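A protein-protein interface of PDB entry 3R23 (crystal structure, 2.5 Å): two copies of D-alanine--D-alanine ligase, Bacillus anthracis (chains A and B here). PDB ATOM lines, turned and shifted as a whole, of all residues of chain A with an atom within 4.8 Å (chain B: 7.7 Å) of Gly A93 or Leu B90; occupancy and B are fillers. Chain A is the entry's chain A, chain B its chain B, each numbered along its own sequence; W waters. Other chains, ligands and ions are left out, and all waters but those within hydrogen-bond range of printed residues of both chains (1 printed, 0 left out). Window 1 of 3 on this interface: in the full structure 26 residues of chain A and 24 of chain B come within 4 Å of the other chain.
NZ of Lys B243 is in salt-bridge range of OD2 of Asp A97 (2.9 Å).
OD1 of Asp A97 is in hydrogen-bond range of N of Ile A100 (2.9 Å).
OD1 of Asn B88 lies within hydrogen-bond range of N of Leu B90.
The side-chain hydroxyl (OG) of Ser B91 lies close to the backbone carbonyl oxygen (O) of Lys B243 (3.2 Å).
The side-chain amide oxygen of Gln B74 sits close to the backbone carbonyl oxygen of Gly B71, at 3.3 Å.
N of Asp A70 lies close to SD of Met A96 (3.7 Å).
Asp A70 touches Met B89.
Asp B70 touches Met A89.
Gly B71 touches Met A89.
Met B89 touches Met A89.
CD1 of Leu A90 touches C of Gly B93, 3.8 Å away.
Leu A90 touches Ile B94.
CD1 of Leu B90 touches C of Gly A93, at 3.7 Å.
Ile B100 touches Ile A94 (CG2 to CD1, 3.9 Å).
CD2 of Leu B90 touches OD2 of Asp A97 (3.5 Å).
Ile A100 touches Lys B243.
Gly A93 touches one residue of chain B.
Leu B90 touches three residues of chain A.
Of the printed residues of chain B, Ile A94 touches Leu B90 and Ile B100.
Printed residues of chain A within 4 Å of Ile B94: Leu A90.
Printed residues of chain A within 4 Å of Lys B243: Asp A97 and Ile A100.
Gln B74 touches none of the printed residues of chain A.
The nearest printed residue of chain B that does not touch Gly A93 is Met B89 (6.6 Å).
The nearest residue of chain A that does not touch Leu B90 is Ile A100 (4.7 Å).
The nearest printed residue of chain A that does not touch Ile B104 is Ile A94 (6.2 Å).
Printed residues of chain A that touch a printed residue of chain B: Asp A70, Met A89, Leu A90, Gly A93, Ile A94, Asp A97 and Ile A100.
Hydrophobic or aromatic side chains of chain A that line the printed part of chain B: Met A89, Leu A90, Ile A94 and Ile A100.
Among the printed residues, Asp or Glu carboxylates within 4 Å of a Lys or Arg side-chain nitrogen of the other chain: Asp A97 with Lys B243.
Asp A70 touches Met B89, and with the chains exchanged Met A89 touches Asp B70.
Leu A90 touches Gly B93, and with the chains exchanged Gly A93 touches Leu B90.
Leu A90 touches Ile B94, and with the chains exchanged Ile A94 touches Leu B90.
Ile A94 touches Ile B100, but with the chains exchanged Ile A100 does not touch Ile B94 (4.1 Å).
11 positions are printed for both chains.
Of the 13 pairs that touch across the chains among the printed residues, 7 have their exchanged pair printed and touching as well.
Water W1 lies within hydrogen-bond range of the side-chain carboxylate (OE2) of Glu B78 (2.5 Å) and the side-chain carboxylate (OD2) of Asp A70 (2.7 Å).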
ATOM      1  N   GLU A  69     -27.309   4.145  18.125  1.00  0.00           N
ATOM      2  CA  GLU A  69     -26.428   4.957  18.995  1.00  0.00           C
ATOM      3  C   GLU A  69     -24.913   4.991  18.720  1.00  0.00           C
ATOM      4  O   GLU A  69     -24.241   5.977  19.050  1.00  0.00           O
ATOM      5  CB  GLU A  69     -26.607   4.570  20.456  1.00  0.00           C
ATOM      6  CG  GLU A  69     -28.015   4.763  20.937  1.00  0.00           C
ATOM      7  CD  GLU A  69     -28.235   4.390  22.392  1.00  0.00           C
ATOM      8  OE1 GLU A  69     -27.463   3.565  22.956  1.00  0.00           O
ATOM      9  OE2 GLU A  69     -29.202   4.942  22.958  1.00  0.00           O
ATOM     10  N   ASP A  70     -24.345   3.919  18.187  1.00  0.00           N
ATOM     11  CA  ASP A  70     -22.887   3.879  18.180  1.00  0.00           C
ATOM     12  C   ASP A  70     -22.300   4.812  17.100  1.00  0.00           C
ATOM     13  O   ASP A  70     -21.150   5.259  17.213  1.00  0.00           O
ATOM     14  CB  ASP A  70     -22.313   2.444  18.188  1.00  0.00           C
ATOM     15  CG  ASP A  70     -22.423   1.740  16.849  1.00  0.00           C
ATOM     16  OD1 ASP A  70     -22.655   2.411  15.839  1.00  0.00           O
ATOM     17  OD2 ASP A  70     -22.223   0.507  16.800  1.00  0.00           O
ATOM     18  N   MET A  89     -22.507  11.229  14.019  1.00  0.00           N
ATOM     19  CA  MET A  89     -21.773  10.055  14.495  1.00  0.00           C
ATOM     20  C   MET A  89     -21.017  10.330  15.802  1.00  0.00           C
ATOM     21  O   MET A  89     -21.193   9.612  16.788  1.00  0.00           O
ATOM     22  CB  MET A  89     -20.878   9.490  13.392  1.00  0.00           C
ATOM     23  CG  MET A  89     -19.801   8.487  13.874  1.00  0.00           C
ATOM     24  SD  MET A  89     -18.717   7.894  12.300  1.00  0.00           S
ATOM     25  CE  MET A  89     -18.357   9.625  11.433  1.00  0.00           C
ATOM     26  N   LEU A  90     -20.236  11.407  15.838  1.00  0.00           N
ATOM     27  CA  LEU A  90     -19.466  11.721  17.035  1.00  0.00           C
ATOM     28  C   LEU A  90     -20.350  11.922  18.284  1.00  0.00           C
ATOM     29  O   LEU A  90     -20.087  11.356  19.353  1.00  0.00           O
ATOM     30  CB  LEU A  90     -18.611  12.963  16.814  1.00  0.00           C
ATOM     31  CG  LEU A  90     -17.720  13.302  18.018  1.00  0.00           C
ATOM     32  CD1 LEU A  90     -16.752  12.169  18.298  1.00  0.00           C
ATOM     33  CD2 LEU A  90     -16.984  14.592  17.806  1.00  0.00           C
ATOM     34  N   SER A  91     -21.375  12.753  18.136  1.00  0.00           N
ATOM     35  CA  SER A  91     -22.270  13.070  19.211  1.00  0.00           C
ATOM     36  C   SER A  91     -23.009  11.823  19.724  1.00  0.00           C
ATOM     37  O   SER A  91     -23.257  11.703  20.929  1.00  0.00           O
ATOM     38  CB  SER A  91     -23.253  14.152  18.778  1.00  0.00           C
ATOM     39  OG  SER A  91     -24.282  14.325  19.749  1.00  0.00           O
ATOM     40  N   SER A  92     -23.331  10.891  18.828  1.00  0.00           N
ATOM     41  CA  SER A  92     -24.019   9.663  19.238  1.00  0.00           C
ATOM     42  C   SER A  92     -23.044   8.810  20.020  1.00  0.00           C
ATOM     43  O   SER A  92     -23.353   8.356  21.116  1.00  0.00           O
ATOM     44  CB  SER A  92     -24.543   8.868  18.038  1.00  0.00           C
ATOM     45  OG  SER A  92     -25.313   9.668  17.161  1.00  0.00           O
ATOM     46  N   GLY A  93     -21.862   8.614  19.450  1.00  0.00           N
ATOM     47  CA  GLY A  93     -20.841   7.809  20.069  1.00  0.00           C
ATOM     48  C   GLY A  93     -20.522   8.239  21.492  1.00  0.00           C
ATOM     49  O   GLY A  93     -20.419   7.383  22.388  1.00  0.00           O
ATOM     50  N   ILE A  94     -20.371   9.556  21.688  1.00  0.00           N
ATOM     51  CA  ILE A  94     -20.088  10.156  22.987  1.00  0.00           C
ATOM     52  C   ILE A  94     -21.204   9.970  23.973  1.00  0.00           C
ATOM     53  O   ILE A  94     -20.967   9.570  25.106  1.00  0.00           O
ATOM     54  CB  ILE A  94     -19.902  11.643  22.861  1.00  0.00           C
ATOM     55  CG1 ILE A  94     -18.480  11.960  22.456  1.00  0.00           C
ATOM     56  CG2 ILE A  94     -20.154  12.350  24.177  1.00  0.00           C
ATOM     57  CD1 ILE A  94     -18.274  13.460  22.510  1.00  0.00           C
ATOM     58  N   CYS A  95     -22.423  10.279  23.544  1.00  0.00           N
ATOM     59  CA  CYS A  95     -23.591  10.140  24.392  1.00  0.00           C
ATOM     60  C   CYS A  95     -23.836   8.677  24.729  1.00  0.00           C
ATOM     61  O   CYS A  95     -24.436   8.373  25.741  1.00  0.00           O
ATOM     62  CB  CYS A  95     -24.830  10.724  23.715  1.00  0.00           C
ATOM     63  SG  CYS A  95     -24.787  12.451  23.642  1.00  0.00           S
ATOM     64  N   MET A  96     -23.396   7.756  23.883  1.00  0.00           N
ATOM     65  CA  MET A  96     -23.558   6.338  24.229  1.00  0.00           C
ATOM     66  C   MET A  96     -22.504   5.883  25.253  1.00  0.00           C
ATOM     67  O   MET A  96     -22.616   4.817  25.816  1.00  0.00           O
ATOM     68  CB  MET A  96     -23.441   5.470  22.997  1.00  0.00           C
ATOM     69  CG  MET A  96     -23.894   4.031  23.215  1.00  0.00           C
ATOM     70  SD  MET A  96     -23.616   2.826  21.653  1.00  0.00           S
ATOM     71  CE  MET A  96     -21.675   2.608  21.770  1.00  0.00           C
ATOM     72  N   ASP A  97     -21.471   6.682  25.484  1.00  0.00           N
ATOM     73  CA  ASP A  97     -20.404   6.243  26.348  1.00  0.00           C
ATOM     74  C   ASP A  97     -20.479   7.023  27.665  1.00  0.00           C
ATOM     75  O   ASP A  97     -20.224   8.230  27.751  1.00  0.00           O
ATOM     76  CB  ASP A  97     -19.063   6.421  25.648  1.00  0.00           C
ATOM     77  CG  ASP A  97     -17.902   5.834  26.431  1.00  0.00           C
ATOM     78  OD1 ASP A  97     -17.602   6.366  27.527  1.00  0.00           O
ATOM     79  OD2 ASP A  97     -17.254   4.877  25.919  1.00  0.00           O
ATOM     80  N   ILE A 100     -17.089   8.758  29.069  1.00  0.00           N
ATOM     81  CA  ILE A 100     -16.698   9.943  28.299  1.00  0.00           C
ATOM     82  C   ILE A 100     -17.721  11.058  28.496  1.00  0.00           C
ATOM     83  O   ILE A 100     -17.353  12.213  28.728  1.00  0.00           O
ATOM     84  CB  ILE A 100     -16.562   9.660  26.796  1.00  0.00           C
ATOM     85  CG1 ILE A 100     -15.503   8.582  26.486  1.00  0.00           C
ATOM     86  CG2 ILE A 100     -16.346  10.965  26.035  1.00  0.00           C
ATOM     87  CD1 ILE A 100     -14.089   8.923  26.948  1.00  0.00           C
ATOM     88  N   GLU B  69      -9.688   9.094   9.983  1.00  0.00           N
ATOM     89  CA  GLU B  69      -9.818   9.489  11.384  1.00  0.00           C
ATOM     90  C   GLU B  69     -11.233   9.770  11.877  1.00  0.00           C
ATOM     91  O   GLU B  69     -11.441   9.899  13.070  1.00  0.00           O
ATOM     92  CB  GLU B  69      -8.950  10.727  11.690  1.00  0.00           C
ATOM     93  CG  GLU B  69      -7.495  10.568  11.335  1.00  0.00           C
ATOM     94  CD  GLU B  69      -6.696  11.865  11.476  1.00  0.00           C
ATOM     95  OE1 GLU B  69      -7.292  12.971  11.433  1.00  0.00           O
ATOM     96  OE2 GLU B  69      -5.461  11.759  11.655  1.00  0.00           O
ATOM     97  N   ASP B  70     -12.216   9.876  10.996  1.00  0.00           N
ATOM     98  CA  ASP B  70     -13.501  10.291  11.518  1.00  0.00           C
ATOM     99  C   ASP B  70     -14.217   9.131  12.258  1.00  0.00           C
ATOM    100  O   ASP B  70     -15.080   9.347  13.110  1.00  0.00           O
ATOM    101  CB  ASP B  70     -14.353  11.014  10.465  1.00  0.00           C
ATOM    102  CG  ASP B  70     -14.921  10.095   9.329  1.00  0.00           C
ATOM    103  OD1 ASP B  70     -14.778   8.856   9.319  1.00  0.00           O
ATOM    104  OD2 ASP B  70     -15.562  10.676   8.428  1.00  0.00           O
ATOM    105  N   GLY B  71     -13.808   7.907  11.948  1.00  0.00           N
ATOM    106  CA  GLY B  71     -14.404   6.740  12.554  1.00  0.00           C
ATOM    107  C   GLY B  71     -15.354   5.908  11.691  1.00  0.00           C
ATOM    108  O   GLY B  71     -15.652   4.768  12.080  1.00  0.00           O
ATOM    109  N   GLN B  74     -13.748   2.528  10.431  1.00  0.00           N
ATOM    110  CA  GLN B  74     -13.654   1.617  11.565  1.00  0.00           C
ATOM    111  C   GLN B  74     -15.039   1.080  11.971  1.00  0.00           C
ATOM    112  O   GLN B  74     -15.169  -0.071  12.407  1.00  0.00           O
ATOM    113  CB  GLN B  74     -12.997   2.295  12.776  1.00  0.00           C
ATOM    114  CG  GLN B  74     -11.577   2.692  12.581  1.00  0.00           C
ATOM    115  CD  GLN B  74     -11.434   3.984  11.838  1.00  0.00           C
ATOM    116  OE1 GLN B  74     -12.428   4.608  11.482  1.00  0.00           O
ATOM    117  NE2 GLN B  74     -10.193   4.398  11.595  1.00  0.00           N
ATOM    118  N   GLY B  75     -16.058   1.933  11.869  1.00  0.00           N
ATOM    119  CA  GLY B  75     -17.406   1.555  12.261  1.00  0.00           C
ATOM    120  C   GLY B  75     -17.971   0.514  11.304  1.00  0.00           C
ATOM    121  O   GLY B  75     -18.633  -0.448  11.695  1.00  0.00           O
ATOM    122  N   GLU B  78     -16.089  -2.877  11.759  1.00  0.00           N
ATOM    123  CA  GLU B  78     -16.661  -3.499  12.921  1.00  0.00           C
ATOM    124  C   GLU B  78     -17.964  -4.217  12.581  1.00  0.00           C
ATOM    125  O   GLU B  78     -18.160  -5.344  12.995  1.00  0.00           O
ATOM    126  CB  GLU B  78     -16.934  -2.441  13.974  1.00  0.00           C
ATOM    127  CG  GLU B  78     -17.309  -2.991  15.337  1.00  0.00           C
ATOM    128  CD  GLU B  78     -17.583  -1.870  16.335  1.00  0.00           C
ATOM    129  OE1 GLU B  78     -16.798  -1.699  17.306  1.00  0.00           O
ATOM    130  OE2 GLU B  78     -18.578  -1.138  16.134  1.00  0.00           O
ATOM    131  N   TYR B  84      -9.340  -4.900  12.116  1.00  0.00           N
ATOM    132  CA  TYR B  84      -8.715  -3.836  11.362  1.00  0.00           C
ATOM    133  C   TYR B  84      -7.706  -3.169  12.296  1.00  0.00           C
ATOM    134  O   TYR B  84      -7.768  -3.342  13.511  1.00  0.00           O
ATOM    135  CB  TYR B  84      -9.790  -2.834  10.882  1.00  0.00           C
ATOM    136  CG  TYR B  84     -10.534  -2.219  12.025  1.00  0.00           C
ATOM    137  CD1 TYR B  84     -11.779  -2.689  12.412  1.00  0.00           C
ATOM    138  CD2 TYR B  84      -9.981  -1.180  12.748  1.00  0.00           C
ATOM    139  CE1 TYR B  84     -12.458  -2.114  13.499  1.00  0.00           C
ATOM    140  CE2 TYR B  84     -10.648  -0.609  13.826  1.00  0.00           C
ATOM    141  CZ  TYR B  84     -11.881  -1.093  14.193  1.00  0.00           C
ATOM    142  OH  TYR B  84     -12.531  -0.539  15.254  1.00  0.00           O
ATOM    143  N   SER B  87      -6.952   2.453  16.320  1.00  0.00           N
ATOM    144  CA  SER B  87      -7.985   2.819  17.242  1.00  0.00           C
ATOM    145  C   SER B  87      -9.378   2.555  16.662  1.00  0.00           C
ATOM    146  O   SER B  87      -9.560   2.474  15.437  1.00  0.00           O
ATOM    147  CB  SER B  87      -7.823   4.281  17.623  1.00  0.00           C
ATOM    148  OG  SER B  87      -6.677   4.415  18.424  1.00  0.00           O
ATOM    149  N   ASN B  88     -10.358   2.387  17.547  1.00  0.00           N
ATOM    150  CA  ASN B  88     -11.738   2.205  17.091  1.00  0.00           C
ATOM    151  C   ASN B  88     -12.463   3.496  16.743  1.00  0.00           C
ATOM    152  O   ASN B  88     -11.899   4.590  16.837  1.00  0.00           O
ATOM    153  CB  ASN B  88     -12.560   1.360  18.070  1.00  0.00           C
ATOM    154  CG  ASN B  88     -12.847   2.065  19.384  1.00  0.00           C
ATOM    155  OD1 ASN B  88     -12.896   3.286  19.469  1.00  0.00           O
ATOM    156  ND2 ASN B  88     -13.072   1.273  20.422  1.00  0.00           N
ATOM    157  N   MET B  89     -13.719   3.353  16.346  1.00  0.00           N
ATOM    158  CA  MET B  89     -14.539   4.479  15.902  1.00  0.00           C
ATOM    159  C   MET B  89     -14.653   5.617  16.902  1.00  0.00           C
ATOM    160  O   MET B  89     -14.493   6.772  16.549  1.00  0.00           O
ATOM    161  CB  MET B  89     -15.936   4.000  15.577  1.00  0.00           C
ATOM    162  CG  MET B  89     -16.859   5.130  15.102  1.00  0.00           C
ATOM    163  SD  MET B  89     -18.582   4.507  14.359  1.00  0.00           S
ATOM    164  CE  MET B  89     -19.134   3.172  15.677  1.00  0.00           C
ATOM    165  N   LEU B  90     -14.954   5.296  18.150  1.00  0.00           N
ATOM    166  CA  LEU B  90     -15.206   6.340  19.112  1.00  0.00           C
ATOM    167  C   LEU B  90     -13.902   7.088  19.413  1.00  0.00           C
ATOM    168  O   LEU B  90     -13.871   8.328  19.431  1.00  0.00           O
ATOM    169  CB  LEU B  90     -15.791   5.743  20.371  1.00  0.00           C
ATOM    170  CG  LEU B  90     -16.004   6.756  21.480  1.00  0.00           C
ATOM    171  CD1 LEU B  90     -16.907   7.865  21.002  1.00  0.00           C
ATOM    172  CD2 LEU B  90     -16.565   6.061  22.716  1.00  0.00           C
ATOM    173  N   SER B  91     -12.833   6.320  19.620  1.00  0.00           N
ATOM    174  CA  SER B  91     -11.520   6.867  19.865  1.00  0.00           C
ATOM    175  C   SER B  91     -10.944   7.700  18.687  1.00  0.00           C
ATOM    176  O   SER B  91     -10.433   8.803  18.898  1.00  0.00           O
ATOM    177  CB  SER B  91     -10.578   5.749  20.249  1.00  0.00           C
ATOM    178  OG  SER B  91      -9.295   6.281  20.492  1.00  0.00           O
ATOM    179  N   SER B  92     -11.026   7.185  17.457  1.00  0.00           N
ATOM    180  CA  SER B  92     -10.685   7.995  16.281  1.00  0.00           C
ATOM    181  C   SER B  92     -11.444   9.311  16.243  1.00  0.00           C
ATOM    182  O   SER B  92     -10.871  10.363  16.077  1.00  0.00           O
ATOM    183  CB  SER B  92     -10.989   7.244  15.012  1.00  0.00           C
ATOM    184  OG  SER B  92     -10.307   6.021  15.012  1.00  0.00           O
ATOM    185  N   GLY B  93     -12.747   9.253  16.403  1.00  0.00           N
ATOM    186  CA  GLY B  93     -13.564  10.449  16.358  1.00  0.00           C
ATOM    187  C   GLY B  93     -13.173  11.477  17.386  1.00  0.00           C
ATOM    188  O   GLY B  93     -13.012  12.647  17.059  1.00  0.00           O
ATOM    189  N   ILE B  94     -13.035  11.033  18.634  1.00  0.00           N
ATOM    190  CA  ILE B  94     -12.705  11.900  19.755  1.00  0.00           C
ATOM    191  C   ILE B  94     -11.337  12.557  19.537  1.00  0.00           C
ATOM    192  O   ILE B  94     -11.137  13.736  19.834  1.00  0.00           O
ATOM    193  CB  ILE B  94     -12.704  11.077  21.073  1.00  0.00           C
ATOM    194  CG1 ILE B  94     -14.131  10.818  21.547  1.00  0.00           C
ATOM    195  CG2 ILE B  94     -11.925  11.770  22.171  1.00  0.00           C
ATOM    196  CD1 ILE B  94     -14.190   9.840  22.684  1.00  0.00           C
ATOM    197  N   CYS B  95     -10.394  11.783  19.012  1.00  0.00           N
ATOM    198  CA  CYS B  95      -9.034  12.276  18.815  1.00  0.00           C
ATOM    199  C   CYS B  95      -8.926  13.255  17.660  1.00  0.00           C
ATOM    200  O   CYS B  95      -7.940  13.952  17.521  1.00  0.00           O
ATOM    201  CB  CYS B  95      -8.056  11.120  18.597  1.00  0.00           C
ATOM    202  SG  CYS B  95      -7.812  10.195  20.117  1.00  0.00           S
ATOM    203  N   MET B  96      -9.937  13.269  16.814  1.00  0.00           N
ATOM    204  CA  MET B  96      -9.982  14.198  15.712  1.00  0.00           C
ATOM    205  C   MET B  96     -10.732  15.471  16.105  1.00  0.00           C
ATOM    206  O   MET B  96     -10.721  16.447  15.368  1.00  0.00           O
ATOM    207  CB  MET B  96     -10.680  13.555  14.529  1.00  0.00           C
ATOM    208  CG  MET B  96     -10.863  14.535  13.401  1.00  0.00           C
ATOM    209  SD  MET B  96     -11.739  13.788  11.868  1.00  0.00           S
ATOM    210  CE  MET B  96     -13.545  14.502  12.224  1.00  0.00           C
ATOM    211  N   ILE B 100     -13.312  18.421  22.182  1.00  0.00           N
ATOM    212  CA  ILE B 100     -13.711  17.293  23.045  1.00  0.00           C
ATOM    213  C   ILE B 100     -12.483  16.590  23.641  1.00  0.00           C
ATOM    214  O   ILE B 100     -12.490  16.109  24.777  1.00  0.00           O
ATOM    215  CB  ILE B 100     -14.551  16.239  22.286  1.00  0.00           C
ATOM    216  CG1 ILE B 100     -15.911  16.801  21.827  1.00  0.00           C
ATOM    217  CG2 ILE B 100     -14.710  15.008  23.111  1.00  0.00           C
ATOM    218  CD1 ILE B 100     -16.724  17.429  22.910  1.00  0.00           C
ATOM    219  N   ILE B 104     -11.662  16.007  27.758  1.00  0.00           N
ATOM    220  CA  ILE B 104     -11.311  14.740  28.369  1.00  0.00           C
ATOM    221  C   ILE B 104      -9.883  14.779  28.932  1.00  0.00           C
ATOM    222  O   ILE B 104      -9.597  14.105  29.905  1.00  0.00           O
ATOM    223  CB  ILE B 104     -11.456  13.580  27.377  1.00  0.00           C
ATOM    224  CG1 ILE B 104     -12.866  13.541  26.784  1.00  0.00           C
ATOM    225  CG2 ILE B 104     -11.155  12.271  28.037  1.00  0.00           C
ATOM    226  CD1 ILE B 104     -13.007  12.544  25.633  1.00  0.00           C
ATOM    227  N   LEU B 242      -7.915   8.841  25.903  1.00  0.00           N
ATOM    228  CA  LEU B 242      -8.614   9.048  24.657  1.00  0.00           C
ATOM    229  C   LEU B 242      -9.057   7.732  24.036  1.00  0.00           C
ATOM    230  O   LEU B 242      -9.567   7.702  22.920  1.00  0.00           O
ATOM    231  CB  LEU B 242      -7.774   9.914  23.714  1.00  0.00           C
ATOM    232  CG  LEU B 242      -7.545  11.318  24.271  1.00  0.00           C
ATOM    233  CD1 LEU B 242      -6.863  12.243  23.269  1.00  0.00           C
ATOM    234  CD2 LEU B 242      -8.837  11.938  24.768  1.00  0.00           C
ATOM    235  N   LYS B 243      -8.822   6.647  24.762  1.00  0.00           N
ATOM    236  CA  LYS B 243      -9.257   5.298  24.393  1.00  0.00           C
ATOM    237  C   LYS B 243      -8.603   4.766  23.132  1.00  0.00           C
ATOM    238  O   LYS B 243      -9.118   3.839  22.494  1.00  0.00           O
ATOM    239  CB  LYS B 243     -10.774   5.230  24.230  1.00  0.00           C
ATOM    240  CG  LYS B 243     -11.523   5.740  25.459  1.00  0.00           C
ATOM    241  CD  LYS B 243     -13.028   5.503  25.302  1.00  0.00           C
ATOM    242  CE  LYS B 243     -13.382   4.052  25.563  1.00  0.00           C
ATOM    243  NZ  LYS B 243     -14.743   3.757  25.121  1.00  0.00           N
ATOM    244  N   CYS B 244      -7.439   5.315  22.813  1.00  0.00           N
ATOM    245  CA  CYS B 244      -6.629   4.828  21.707  1.00  0.00           C
ATOM    246  C   CYS B 244      -6.240   3.371  21.877  1.00  0.00           C
ATOM    247  O   CYS B 244      -6.187   2.831  22.981  1.00  0.00           O
ATOM    248  CB  CYS B 244      -5.366   5.661  21.599  1.00  0.00           C
ATOM    249  SG  CYS B 244      -5.755   7.389  21.313  1.00  0.00           S
ATOM    250  N   THR B 266      -4.457   9.177  15.851  1.00  0.00           N
ATOM    251  CA  THR B 266      -4.817   7.767  15.918  1.00  0.00           C
ATOM    252  C   THR B 266      -4.376   7.088  14.642  1.00  0.00           C
ATOM    253  O   THR B 266      -4.322   5.880  14.541  1.00  0.00           O
ATOM    254  CB  THR B 266      -6.330   7.597  16.025  1.00  0.00           C
ATOM    255  OG1 THR B 266      -6.944   8.247  14.902  1.00  0.00           O
ATOM    256  CG2 THR B 266      -6.833   8.231  17.296  1.00  0.00           C
HETATM  257  O   HOH W   1     -20.639  -0.538  14.911  1.00  0.00           O
